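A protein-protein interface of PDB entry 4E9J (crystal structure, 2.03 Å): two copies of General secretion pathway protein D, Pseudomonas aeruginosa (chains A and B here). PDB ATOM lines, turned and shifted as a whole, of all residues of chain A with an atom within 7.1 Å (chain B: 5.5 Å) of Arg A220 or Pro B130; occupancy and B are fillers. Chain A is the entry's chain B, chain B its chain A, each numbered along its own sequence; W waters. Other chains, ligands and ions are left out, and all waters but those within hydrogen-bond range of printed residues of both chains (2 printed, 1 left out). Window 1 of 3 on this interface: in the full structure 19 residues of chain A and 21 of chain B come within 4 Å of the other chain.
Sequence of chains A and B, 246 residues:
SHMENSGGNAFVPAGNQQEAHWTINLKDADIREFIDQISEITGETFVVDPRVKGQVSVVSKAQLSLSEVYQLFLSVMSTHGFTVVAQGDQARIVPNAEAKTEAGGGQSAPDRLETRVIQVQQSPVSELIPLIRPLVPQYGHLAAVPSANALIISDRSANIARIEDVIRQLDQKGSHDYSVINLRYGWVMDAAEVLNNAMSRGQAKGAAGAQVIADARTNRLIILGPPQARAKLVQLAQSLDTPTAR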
ATOM      1  N   PRO A 130      33.924  24.801   5.318  1.00  0.00           N
ATOM      2  CA  PRO A 130      32.681  24.053   5.060  1.00  0.00           C
ATOM      3  C   PRO A 130      31.768  24.670   4.004  1.00  0.00           C
ATOM      4  O   PRO A 130      31.004  23.953   3.367  1.00  0.00           O
ATOM      5  CB  PRO A 130      31.963  24.071   6.424  1.00  0.00           C
ATOM      6  CG  PRO A 130      32.959  24.406   7.391  1.00  0.00           C
ATOM      7  CD  PRO A 130      33.992  25.226   6.726  1.00  0.00           C
ATOM      8  N   PRO A 134      31.586  22.226  -0.710  1.00  0.00           N
ATOM      9  CA  PRO A 134      30.645  21.770  -1.749  1.00  0.00           C
ATOM     10  C   PRO A 134      31.025  22.042  -3.205  1.00  0.00           C
ATOM     11  O   PRO A 134      30.577  21.340  -4.109  1.00  0.00           O
ATOM     12  CB  PRO A 134      29.388  22.572  -1.426  1.00  0.00           C
ATOM     13  CG  PRO A 134      29.442  22.816   0.068  1.00  0.00           C
ATOM     14  CD  PRO A 134      30.898  23.037   0.320  1.00  0.00           C
ATOM     15  N   TYR A 178      23.643  30.893   8.397  1.00  0.00           N
ATOM     16  CA  TYR A 178      23.121  30.374   7.135  1.00  0.00           C
ATOM     17  C   TYR A 178      22.029  29.398   7.308  1.00  0.00           C
ATOM     18  O   TYR A 178      21.761  28.923   8.397  1.00  0.00           O
ATOM     19  CB  TYR A 178      24.259  29.757   6.296  1.00  0.00           C
ATOM     20  CG  TYR A 178      24.961  28.582   6.951  1.00  0.00           C
ATOM     21  CD1 TYR A 178      24.540  27.275   6.722  1.00  0.00           C
ATOM     22  CD2 TYR A 178      26.086  28.773   7.741  1.00  0.00           C
ATOM     23  CE1 TYR A 178      25.232  26.186   7.268  1.00  0.00           C
ATOM     24  CE2 TYR A 178      26.837  27.693   8.212  1.00  0.00           C
ATOM     25  CZ  TYR A 178      26.375  26.406   8.029  1.00  0.00           C
ATOM     26  OH  TYR A 178      27.090  25.391   8.619  1.00  0.00           O
ATOM     27  N   VAL A 180      20.267  25.828   5.375  1.00  0.00           N
ATOM     28  CA  VAL A 180      20.445  24.703   4.474  1.00  0.00           C
ATOM     29  C   VAL A 180      19.086  24.166   4.039  1.00  0.00           C
ATOM     30  O   VAL A 180      18.228  23.932   4.881  1.00  0.00           O
ATOM     31  CB  VAL A 180      21.316  23.619   5.136  1.00  0.00           C
ATOM     32  CG1 VAL A 180      21.354  22.348   4.300  1.00  0.00           C
ATOM     33  CG2 VAL A 180      22.716  24.143   5.400  1.00  0.00           C
ATOM     34  N   ILE A 181      18.905  23.973   2.723  1.00  0.00           N
ATOM     35  CA  ILE A 181      17.673  23.436   2.135  1.00  0.00           C
ATOM     36  C   ILE A 181      18.043  22.216   1.327  1.00  0.00           C
ATOM     37  O   ILE A 181      18.721  22.348   0.328  1.00  0.00           O
ATOM     38  CB  ILE A 181      16.923  24.472   1.242  1.00  0.00           C
ATOM     39  CG1 ILE A 181      16.578  25.757   1.992  1.00  0.00           C
ATOM     40  CG2 ILE A 181      15.668  23.841   0.665  1.00  0.00           C
ATOM     41  CD1 ILE A 181      16.202  26.884   1.117  1.00  0.00           C
ATOM     42  N   ASN A 182      17.556  21.051   1.740  1.00  0.00           N
ATOM     43  CA  ASN A 182      17.737  19.774   1.050  1.00  0.00           C
ATOM     44  C   ASN A 182      16.617  19.678   0.054  1.00  0.00           C
ATOM     45  O   ASN A 182      15.479  19.497   0.449  1.00  0.00           O
ATOM     46  CB  ASN A 182      17.641  18.601   2.013  1.00  0.00           C
ATOM     47  CG  ASN A 182      18.668  18.670   3.087  1.00  0.00           C
ATOM     48  OD1 ASN A 182      19.817  18.319   2.876  1.00  0.00           O
ATOM     49  ND2 ASN A 182      18.313  19.203   4.229  1.00  0.00           N
ATOM     50  N   LEU A 183      16.923  19.833  -1.211  1.00  0.00           N
ATOM     51  CA  LEU A 183      15.883  19.864  -2.235  1.00  0.00           C
ATOM     52  C   LEU A 183      15.307  18.466  -2.454  1.00  0.00           C
ATOM     53  O   LEU A 183      16.025  17.484  -2.341  1.00  0.00           O
ATOM     54  CB  LEU A 183      16.414  20.462  -3.563  1.00  0.00           C
ATOM     55  CG  LEU A 183      16.812  21.957  -3.565  1.00  0.00           C
ATOM     56  CD1 LEU A 183      17.305  22.377  -4.959  1.00  0.00           C
ATOM     57  CD2 LEU A 183      15.641  22.863  -3.251  1.00  0.00           C
ATOM     58  N   TRP A 187      16.594  20.659  -8.813  1.00  0.00           N
ATOM     59  CA  TRP A 187      17.994  20.362  -8.959  1.00  0.00           C
ATOM     60  C   TRP A 187      18.789  21.609  -8.550  1.00  0.00           C
ATOM     61  O   TRP A 187      18.536  22.703  -9.076  1.00  0.00           O
ATOM     62  CB  TRP A 187      18.296  19.979 -10.394  1.00  0.00           C
ATOM     63  CG  TRP A 187      19.761  19.823 -10.668  1.00  0.00           C
ATOM     64  CD1 TRP A 187      20.486  20.448 -11.637  1.00  0.00           C
ATOM     65  CD2 TRP A 187      20.692  19.038  -9.915  1.00  0.00           C
ATOM     66  NE1 TRP A 187      21.795  20.016 -11.598  1.00  0.00           N
ATOM     67  CE2 TRP A 187      21.961  19.202 -10.514  1.00  0.00           C
ATOM     68  CE3 TRP A 187      20.582  18.212  -8.792  1.00  0.00           C
ATOM     69  CZ2 TRP A 187      23.109  18.594 -10.006  1.00  0.00           C
ATOM     70  CZ3 TRP A 187      21.721  17.568  -8.317  1.00  0.00           C
ATOM     71  CH2 TRP A 187      22.959  17.755  -8.926  1.00  0.00           C
ATOM     72  N   VAL A 188      19.769  21.433  -7.677  1.00  0.00           N
ATOM     73  CA  VAL A 188      20.456  22.568  -7.079  1.00  0.00           C
ATOM     74  C   VAL A 188      21.174  23.473  -8.070  1.00  0.00           C
ATOM     75  O   VAL A 188      21.135  24.672  -7.879  1.00  0.00           O
ATOM     76  CB  VAL A 188      21.429  22.192  -5.937  1.00  0.00           C
ATOM     77  CG1 VAL A 188      20.664  21.696  -4.748  1.00  0.00           C
ATOM     78  CG2 VAL A 188      22.504  21.214  -6.401  1.00  0.00           C
ATOM     79  N   VAL A 212      23.835  32.327  -2.455  1.00  0.00           N
ATOM     80  CA  VAL A 212      23.491  30.906  -2.504  1.00  0.00           C
ATOM     81  C   VAL A 212      24.688  30.099  -2.995  1.00  0.00           C
ATOM     82  O   VAL A 212      25.430  30.530  -3.887  1.00  0.00           O
ATOM     83  CB  VAL A 212      22.182  30.639  -3.302  1.00  0.00           C
ATOM     84  CG1 VAL A 212      22.335  30.950  -4.785  1.00  0.00           C
ATOM     85  CG2 VAL A 212      21.693  29.222  -3.109  1.00  0.00           C
ATOM     86  N   ILE A 213      24.958  28.996  -2.301  1.00  0.00           N
ATOM     87  CA  ILE A 213      26.053  28.086  -2.631  1.00  0.00           C
ATOM     88  C   ILE A 213      25.364  26.741  -2.891  1.00  0.00           C
ATOM     89  O   ILE A 213      24.671  26.221  -2.003  1.00  0.00           O
ATOM     90  CB  ILE A 213      27.107  27.986  -1.509  1.00  0.00           C
ATOM     91  CG1 ILE A 213      27.930  29.297  -1.404  1.00  0.00           C
ATOM     92  CG2 ILE A 213      28.026  26.772  -1.760  1.00  0.00           C
ATOM     93  CD1 ILE A 213      28.842  29.417  -0.185  1.00  0.00           C
ATOM     94  N   ALA A 214      25.486  26.206  -4.110  1.00  0.00           N
ATOM     95  CA  ALA A 214      24.899  24.915  -4.471  1.00  0.00           C
ATOM     96  C   ALA A 214      25.837  23.789  -4.065  1.00  0.00           C
ATOM     97  O   ALA A 214      27.020  23.800  -4.405  1.00  0.00           O
ATOM     98  CB  ALA A 214      24.667  24.852  -5.963  1.00  0.00           C
ATOM     99  N   ASP A 215      25.297  22.808  -3.392  1.00  0.00           N
ATOM    100  CA  ASP A 215      26.036  21.654  -2.927  1.00  0.00           C
ATOM    101  C   ASP A 215      25.422  20.464  -3.670  1.00  0.00           C
ATOM    102  O   ASP A 215      24.463  19.848  -3.199  1.00  0.00           O
ATOM    103  CB  ASP A 215      25.986  21.565  -1.390  1.00  0.00           C
ATOM    104  CG  ASP A 215      26.730  20.393  -0.781  1.00  0.00           C
ATOM    105  OD1 ASP A 215      27.389  19.647  -1.539  1.00  0.00           O
ATOM    106  OD2 ASP A 215      26.700  20.257   0.459  1.00  0.00           O
ATOM    107  N   ALA A 216      25.975  20.210  -4.895  1.00  0.00           N
ATOM    108  CA  ALA A 216      25.525  19.202  -5.867  1.00  0.00           C
ATOM    109  C   ALA A 216      25.623  17.769  -5.375  1.00  0.00           C
ATOM    110  O   ALA A 216      24.798  16.968  -5.788  1.00  0.00           O
ATOM    111  CB  ALA A 216      26.289  19.344  -7.193  1.00  0.00           C
ATOM    112  N   ARG A 217      26.600  17.441  -4.500  1.00  0.00           N
ATOM    113  CA  ARG A 217      26.726  16.080  -3.948  1.00  0.00           C
ATOM    114  C   ARG A 217      25.515  15.608  -3.175  1.00  0.00           C
ATOM    115  O   ARG A 217      25.192  14.430  -3.283  1.00  0.00           O
ATOM    116  CB  ARG A 217      28.014  15.908  -3.098  1.00  0.00           C
ATOM    117  CG  ARG A 217      29.268  15.647  -3.962  1.00  0.00           C
ATOM    118  CD  ARG A 217      30.496  15.312  -3.128  1.00  0.00           C
ATOM    119  NE  ARG A 217      30.949  16.456  -2.323  1.00  0.00           N
ATOM    120  CZ  ARG A 217      31.753  17.439  -2.741  1.00  0.00           C
ATOM    121  NH1 ARG A 217      32.232  17.438  -3.980  1.00  0.00           N
ATOM    122  NH2 ARG A 217      32.088  18.426  -1.917  1.00  0.00           N
ATOM    123  N   THR A 218      24.850  16.488  -2.403  1.00  0.00           N
ATOM    124  CA  THR A 218      23.680  16.113  -1.603  1.00  0.00           C
ATOM    125  C   THR A 218      22.414  16.842  -2.028  1.00  0.00           C
ATOM    126  O   THR A 218      21.381  16.730  -1.349  1.00  0.00           O
ATOM    127  CB  THR A 218      23.997  16.294  -0.110  1.00  0.00           C
ATOM    128  OG1 THR A 218      24.416  17.633   0.121  1.00  0.00           O
ATOM    129  CG2 THR A 218      25.066  15.321   0.365  1.00  0.00           C
ATOM    130  N   ASN A 219      22.453  17.493  -3.202  1.00  0.00           N
ATOM    131  CA  ASN A 219      21.324  18.199  -3.781  1.00  0.00           C
ATOM    132  C   ASN A 219      20.711  19.159  -2.761  1.00  0.00           C
ATOM    133  O   ASN A 219      19.526  19.104  -2.473  1.00  0.00           O
ATOM    134  CB  ASN A 219      20.280  17.234  -4.358  1.00  0.00           C
ATOM    135  CG  ASN A 219      19.371  17.915  -5.376  1.00  0.00           C
ATOM    136  OD1 ASN A 219      19.805  18.743  -6.142  1.00  0.00           O
ATOM    137  ND2 ASN A 219      18.069  17.761  -5.303  1.00  0.00           N
ATOM    138  N   ARG A 220      21.554  20.022  -2.209  1.00  0.00           N
ATOM    139  CA  ARG A 220      21.116  21.014  -1.231  1.00  0.00           C
ATOM    140  C   ARG A 220      21.710  22.412  -1.480  1.00  0.00           C
ATOM    141  O   ARG A 220      22.794  22.552  -2.063  1.00  0.00           O
ATOM    142  CB  ARG A 220      21.446  20.512   0.175  1.00  0.00           C
ATOM    143  CG  ARG A 220      22.882  20.593   0.518  1.00  0.00           C
ATOM    144  CD  ARG A 220      23.182  20.031   1.888  1.00  0.00           C
ATOM    145  NE  ARG A 220      24.572  20.329   2.238  1.00  0.00           N
ATOM    146  CZ  ARG A 220      25.085  20.354   3.462  1.00  0.00           C
ATOM    147  NH1 ARG A 220      26.351  20.688   3.643  1.00  0.00           N
ATOM    148  NH2 ARG A 220      24.331  20.064   4.520  1.00  0.00           N
ATOM    149  N   LEU A 221      21.001  23.429  -1.019  1.00  0.00           N
ATOM    150  CA  LEU A 221      21.410  24.824  -1.133  1.00  0.00           C
ATOM    151  C   LEU A 221      21.843  25.327   0.210  1.00  0.00           C
ATOM    152  O   LEU A 221      21.197  25.035   1.214  1.00  0.00           O
ATOM    153  CB  LEU A 221      20.242  25.710  -1.591  1.00  0.00           C
ATOM    154  CG  LEU A 221      19.621  25.400  -2.926  1.00  0.00           C
ATOM    155  CD1 LEU A 221      18.443  26.320  -3.185  1.00  0.00           C
ATOM    156  CD2 LEU A 221      20.640  25.533  -4.035  1.00  0.00           C
ATOM    157  N   ILE A 222      22.873  26.161   0.220  1.00  0.00           N
ATOM    158  CA  ILE A 222      23.348  26.847   1.418  1.00  0.00           C
ATOM    159  C   ILE A 222      23.064  28.317   1.121  1.00  0.00           C
ATOM    160  O   ILE A 222      23.553  28.821   0.108  1.00  0.00           O
ATOM    161  CB  ILE A 222      24.817  26.562   1.687  1.00  0.00           C
ATOM    162  CG1 ILE A 222      25.038  25.056   1.950  1.00  0.00           C
ATOM    163  CG2 ILE A 222      25.315  27.416   2.831  1.00  0.00           C
ATOM    164  CD1 ILE A 222      26.492  24.599   1.751  1.00  0.00           C
ATOM    165  N   SER B 126      23.535  10.876   4.720  1.00  0.00           N
ATOM    166  CA  SER B 126      24.188  12.161   4.437  1.00  0.00           C
ATOM    167  C   SER B 126      23.478  13.345   5.079  1.00  0.00           C
ATOM    168  O   SER B 126      24.141  14.280   5.479  1.00  0.00           O
ATOM    169  CB  SER B 126      24.301  12.395   2.930  1.00  0.00           C
ATOM    170  OG  SER B 126      23.008  12.430   2.346  1.00  0.00           O
ATOM    171  N   GLU B 127      22.150  13.304   5.202  1.00  0.00           N
ATOM    172  CA  GLU B 127      21.405  14.400   5.816  1.00  0.00           C
ATOM    173  C   GLU B 127      21.563  14.481   7.347  1.00  0.00           C
ATOM    174  O   GLU B 127      21.319  15.547   7.904  1.00  0.00           O
ATOM    175  CB  GLU B 127      19.937  14.314   5.405  1.00  0.00           C
ATOM    176  CG  GLU B 127      19.761  14.522   3.911  1.00  0.00           C
ATOM    177  CD  GLU B 127      18.362  14.322   3.369  1.00  0.00           C
ATOM    178  OE1 GLU B 127      17.448  14.044   4.179  1.00  0.00           O
ATOM    179  OE2 GLU B 127      18.178  14.447   2.133  1.00  0.00           O
ATOM    180  N   LEU B 128      21.929  13.371   8.037  1.00  0.00           N
ATOM    181  CA  LEU B 128      22.108  13.392   9.486  1.00  0.00           C
ATOM    182  C   LEU B 128      23.525  13.815   9.869  1.00  0.00           C
ATOM    183  O   LEU B 128      23.677  14.374  10.944  1.00  0.00           O
ATOM    184  CB  LEU B 128      21.778  12.019  10.111  1.00  0.00           C
ATOM    185  CG  LEU B 128      20.376  11.460   9.812  1.00  0.00           C
ATOM    186  CD1 LEU B 128      20.210  10.101  10.421  1.00  0.00           C
ATOM    187  CD2 LEU B 128      19.259  12.376  10.376  1.00  0.00           C
ATOM    188  N   ILE B 129      24.537  13.602   8.997  1.00  0.00           N
ATOM    189  CA  ILE B 129      25.960  13.908   9.267  1.00  0.00           C
ATOM    190  C   ILE B 129      26.194  15.324   9.865  1.00  0.00           C
ATOM    191  O   ILE B 129      26.833  15.437  10.919  1.00  0.00           O
ATOM    192  CB  ILE B 129      26.838  13.672   7.991  1.00  0.00           C
ATOM    193  CG1 ILE B 129      26.905  12.174   7.561  1.00  0.00           C
ATOM    194  CG2 ILE B 129      28.241  14.308   8.152  1.00  0.00           C
ATOM    195  CD1 ILE B 129      28.107  11.343   7.994  1.00  0.00           C
ATOM    196  N   PRO B 130      25.709  16.430   9.242  1.00  0.00           N
ATOM    197  CA  PRO B 130      25.954  17.754   9.867  1.00  0.00           C
ATOM    198  C   PRO B 130      25.245  17.942  11.214  1.00  0.00           C
ATOM    199  O   PRO B 130      25.661  18.780  12.019  1.00  0.00           O
ATOM    200  CB  PRO B 130      25.507  18.772   8.809  1.00  0.00           C
ATOM    201  CG  PRO B 130      24.974  17.975   7.642  1.00  0.00           C
ATOM    202  CD  PRO B 130      24.905  16.533   8.009  1.00  0.00           C
ATOM    203  N   LEU B 131      24.195  17.145  11.483  1.00  0.00           N
ATOM    204  CA  LEU B 131      23.471  17.258  12.747  1.00  0.00           C
ATOM    205  C   LEU B 131      24.147  16.463  13.877  1.00  0.00           C
ATOM    206  O   LEU B 131      23.924  16.753  15.048  1.00  0.00           O
ATOM    207  CB  LEU B 131      22.039  16.792  12.548  1.00  0.00           C
ATOM    208  CG  LEU B 131      21.310  17.360  11.306  1.00  0.00           C
ATOM    209  CD1 LEU B 131      19.904  16.848  11.257  1.00  0.00           C
ATOM    210  CD2 LEU B 131      21.350  18.888  11.274  1.00  0.00           C
ATOM    211  N   ILE B 132      24.965  15.468  13.539  1.00  0.00           N
ATOM    212  CA  ILE B 132      25.636  14.674  14.566  1.00  0.00           C
ATOM    213  C   ILE B 132      27.108  15.047  14.709  1.00  0.00           C
ATOM    214  O   ILE B 132      27.693  14.735  15.737  1.00  0.00           O
ATOM    215  CB  ILE B 132      25.411  13.144  14.383  1.00  0.00           C
ATOM    216  CG1 ILE B 132      25.918  12.651  13.031  1.00  0.00           C
ATOM    217  CG2 ILE B 132      23.908  12.796  14.575  1.00  0.00           C
ATOM    218  CD1 ILE B 132      26.100  11.184  12.964  1.00  0.00           C
ATOM    219  N   ARG B 133      27.710  15.709  13.714  1.00  0.00           N
ATOM    220  CA  ARG B 133      29.111  16.130  13.825  1.00  0.00           C
ATOM    221  C   ARG B 133      29.408  16.959  15.102  1.00  0.00           C
ATOM    222  O   ARG B 133      30.410  16.641  15.750  1.00  0.00           O
ATOM    223  CB  ARG B 133      29.630  16.847  12.569  1.00  0.00           C
ATOM    224  CG  ARG B 133      31.111  16.570  12.335  1.00  0.00           C
ATOM    225  CD  ARG B 133      31.666  17.295  11.131  1.00  0.00           C
ATOM    226  NE  ARG B 133      31.252  16.720   9.852  1.00  0.00           N
ATOM    227  CZ  ARG B 133      31.761  15.623   9.290  1.00  0.00           C
ATOM    228  NH1 ARG B 133      32.706  14.920   9.911  1.00  0.00           N
ATOM    229  NH2 ARG B 133      31.315  15.208   8.110  1.00  0.00           N
ATOM    230  N   PRO B 134      28.541  17.872  15.615  1.00  0.00           N
ATOM    231  CA  PRO B 134      28.892  18.548  16.889  1.00  0.00           C
ATOM    232  C   PRO B 134      29.118  17.606  18.071  1.00  0.00           C
ATOM    233  O   PRO B 134      29.679  18.016  19.092  1.00  0.00           O
ATOM    234  CB  PRO B 134      27.692  19.471  17.174  1.00  0.00           C
ATOM    235  CG  PRO B 134      26.857  19.465  15.995  1.00  0.00           C
ATOM    236  CD  PRO B 134      27.261  18.384  15.063  1.00  0.00           C
ATOM    237  N   TYR B 178      18.016  22.918   8.048  1.00  0.00           N
ATOM    238  CA  TYR B 178      18.395  23.567   9.296  1.00  0.00           C
ATOM    239  C   TYR B 178      18.912  24.962   9.075  1.00  0.00           C
ATOM    240  O   TYR B 178      19.224  25.301   7.932  1.00  0.00           O
ATOM    241  CB  TYR B 178      19.452  22.703  10.020  1.00  0.00           C
ATOM    242  CG  TYR B 178      20.727  22.452   9.233  1.00  0.00           C
ATOM    243  CD1 TYR B 178      20.843  21.362   8.401  1.00  0.00           C
ATOM    244  CD2 TYR B 178      21.837  23.271   9.384  1.00  0.00           C
ATOM    245  CE1 TYR B 178      22.034  21.065   7.751  1.00  0.00           C
ATOM    246  CE2 TYR B 178      23.032  22.998   8.721  1.00  0.00           C
ATOM    247  CZ  TYR B 178      23.140  21.861   7.943  1.00  0.00           C
ATOM    248  OH  TYR B 178      24.291  21.530   7.274  1.00  0.00           O
ATOM    249  N   ILE B 222      22.290  25.054  16.006  1.00  0.00           N
ATOM    250  CA  ILE B 222      21.726  24.464  14.784  1.00  0.00           C
ATOM    251  C   ILE B 222      20.251  24.270  15.091  1.00  0.00           C
ATOM    252  O   ILE B 222      19.935  23.611  16.067  1.00  0.00           O
ATOM    253  CB  ILE B 222      22.414  23.166  14.421  1.00  0.00           C
ATOM    254  CG1 ILE B 222      23.891  23.418  14.101  1.00  0.00           C
ATOM    255  CG2 ILE B 222      21.705  22.487  13.252  1.00  0.00           C
ATOM    256  CD1 ILE B 222      24.757  22.148  14.197  1.00  0.00           C
HETATM  257  O   HOH W   1      23.986  17.052   4.091  1.00  0.00           O
HETATM  258  O   HOH W   2      26.473  22.898   8.048  1.00  0.00           O
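The backbone carbonyl oxygen of Tyr B178 is in hydrogen-bond range of the backbone NH of Val A180 (2.8 Å). NH2 of Arg A220 sits at hydrogen-bond distance from OH of Tyr B178 (3.1 Å).
The side-chain carboxylate of Asp A215 is in hydrogen-bond range of the side-chain hydroxyl of Thr A218, 3.5 Å away. The guanidinium group (NE) of Arg A220 is in salt-bridge range of the side-chain carboxylate (OD2) of Asp A215, at 2.8 Å. The side-chain hydroxyl of Thr A218 lies close to the guanidinium group of Arg A220, 3.4 Å away.
Among the printed residues, merely in contact across the chains: Arg A220 with Pro B130 (3.8 Å), Asn A182 with Glu B127 (3.9 Å) and Thr A218 with Ser B126 (3.97 Å).
Tyr A178 touches none of the printed residues of chain B. Printed residues of chain B within 4 Å of Thr A218: Ser B126. Arg A220 touches two residues of chain B. Pro B130 touches just one residue of chain A: Arg A220 (3.8 Å). Of the printed residues of chain A, Tyr B178 touches Val A180 (2.8 Å) and Arg A220 (3.1 Å). The nearest printed residue of chain B that does not touch Arg A220 is Ser B126 (5.9 Å). The nearest printed residue of chain A that does not touch Ser B126 is Arg A220 (5.9 Å).
Printed residues of chain A that touch a printed residue of chain B: Val A180, Asn A182, Thr A218 and Arg A220. Hydrophobic or aromatic side chains of chain A within 4 Å of the printed part of chain B: Val A180. Of the 11 printed residues of chain B, 4 touch a printed residue of chain A. Hydrophobic or aromatic side chains of chain B within 4 Å of the printed part of chain A: Pro B130 and Tyr B178.
Positions printed for both chains: 130, 134, 178 and 222.
Water W2 bridges OH of Tyr A178 (2.6 Å) and OH of Tyr B178 (2.7 Å). Water W1 bridges the guanidinium group (NH2) of Arg A220 (3.1 Å) and the backbone carbonyl oxygen (O) of Ser B126 (3.1 Å).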
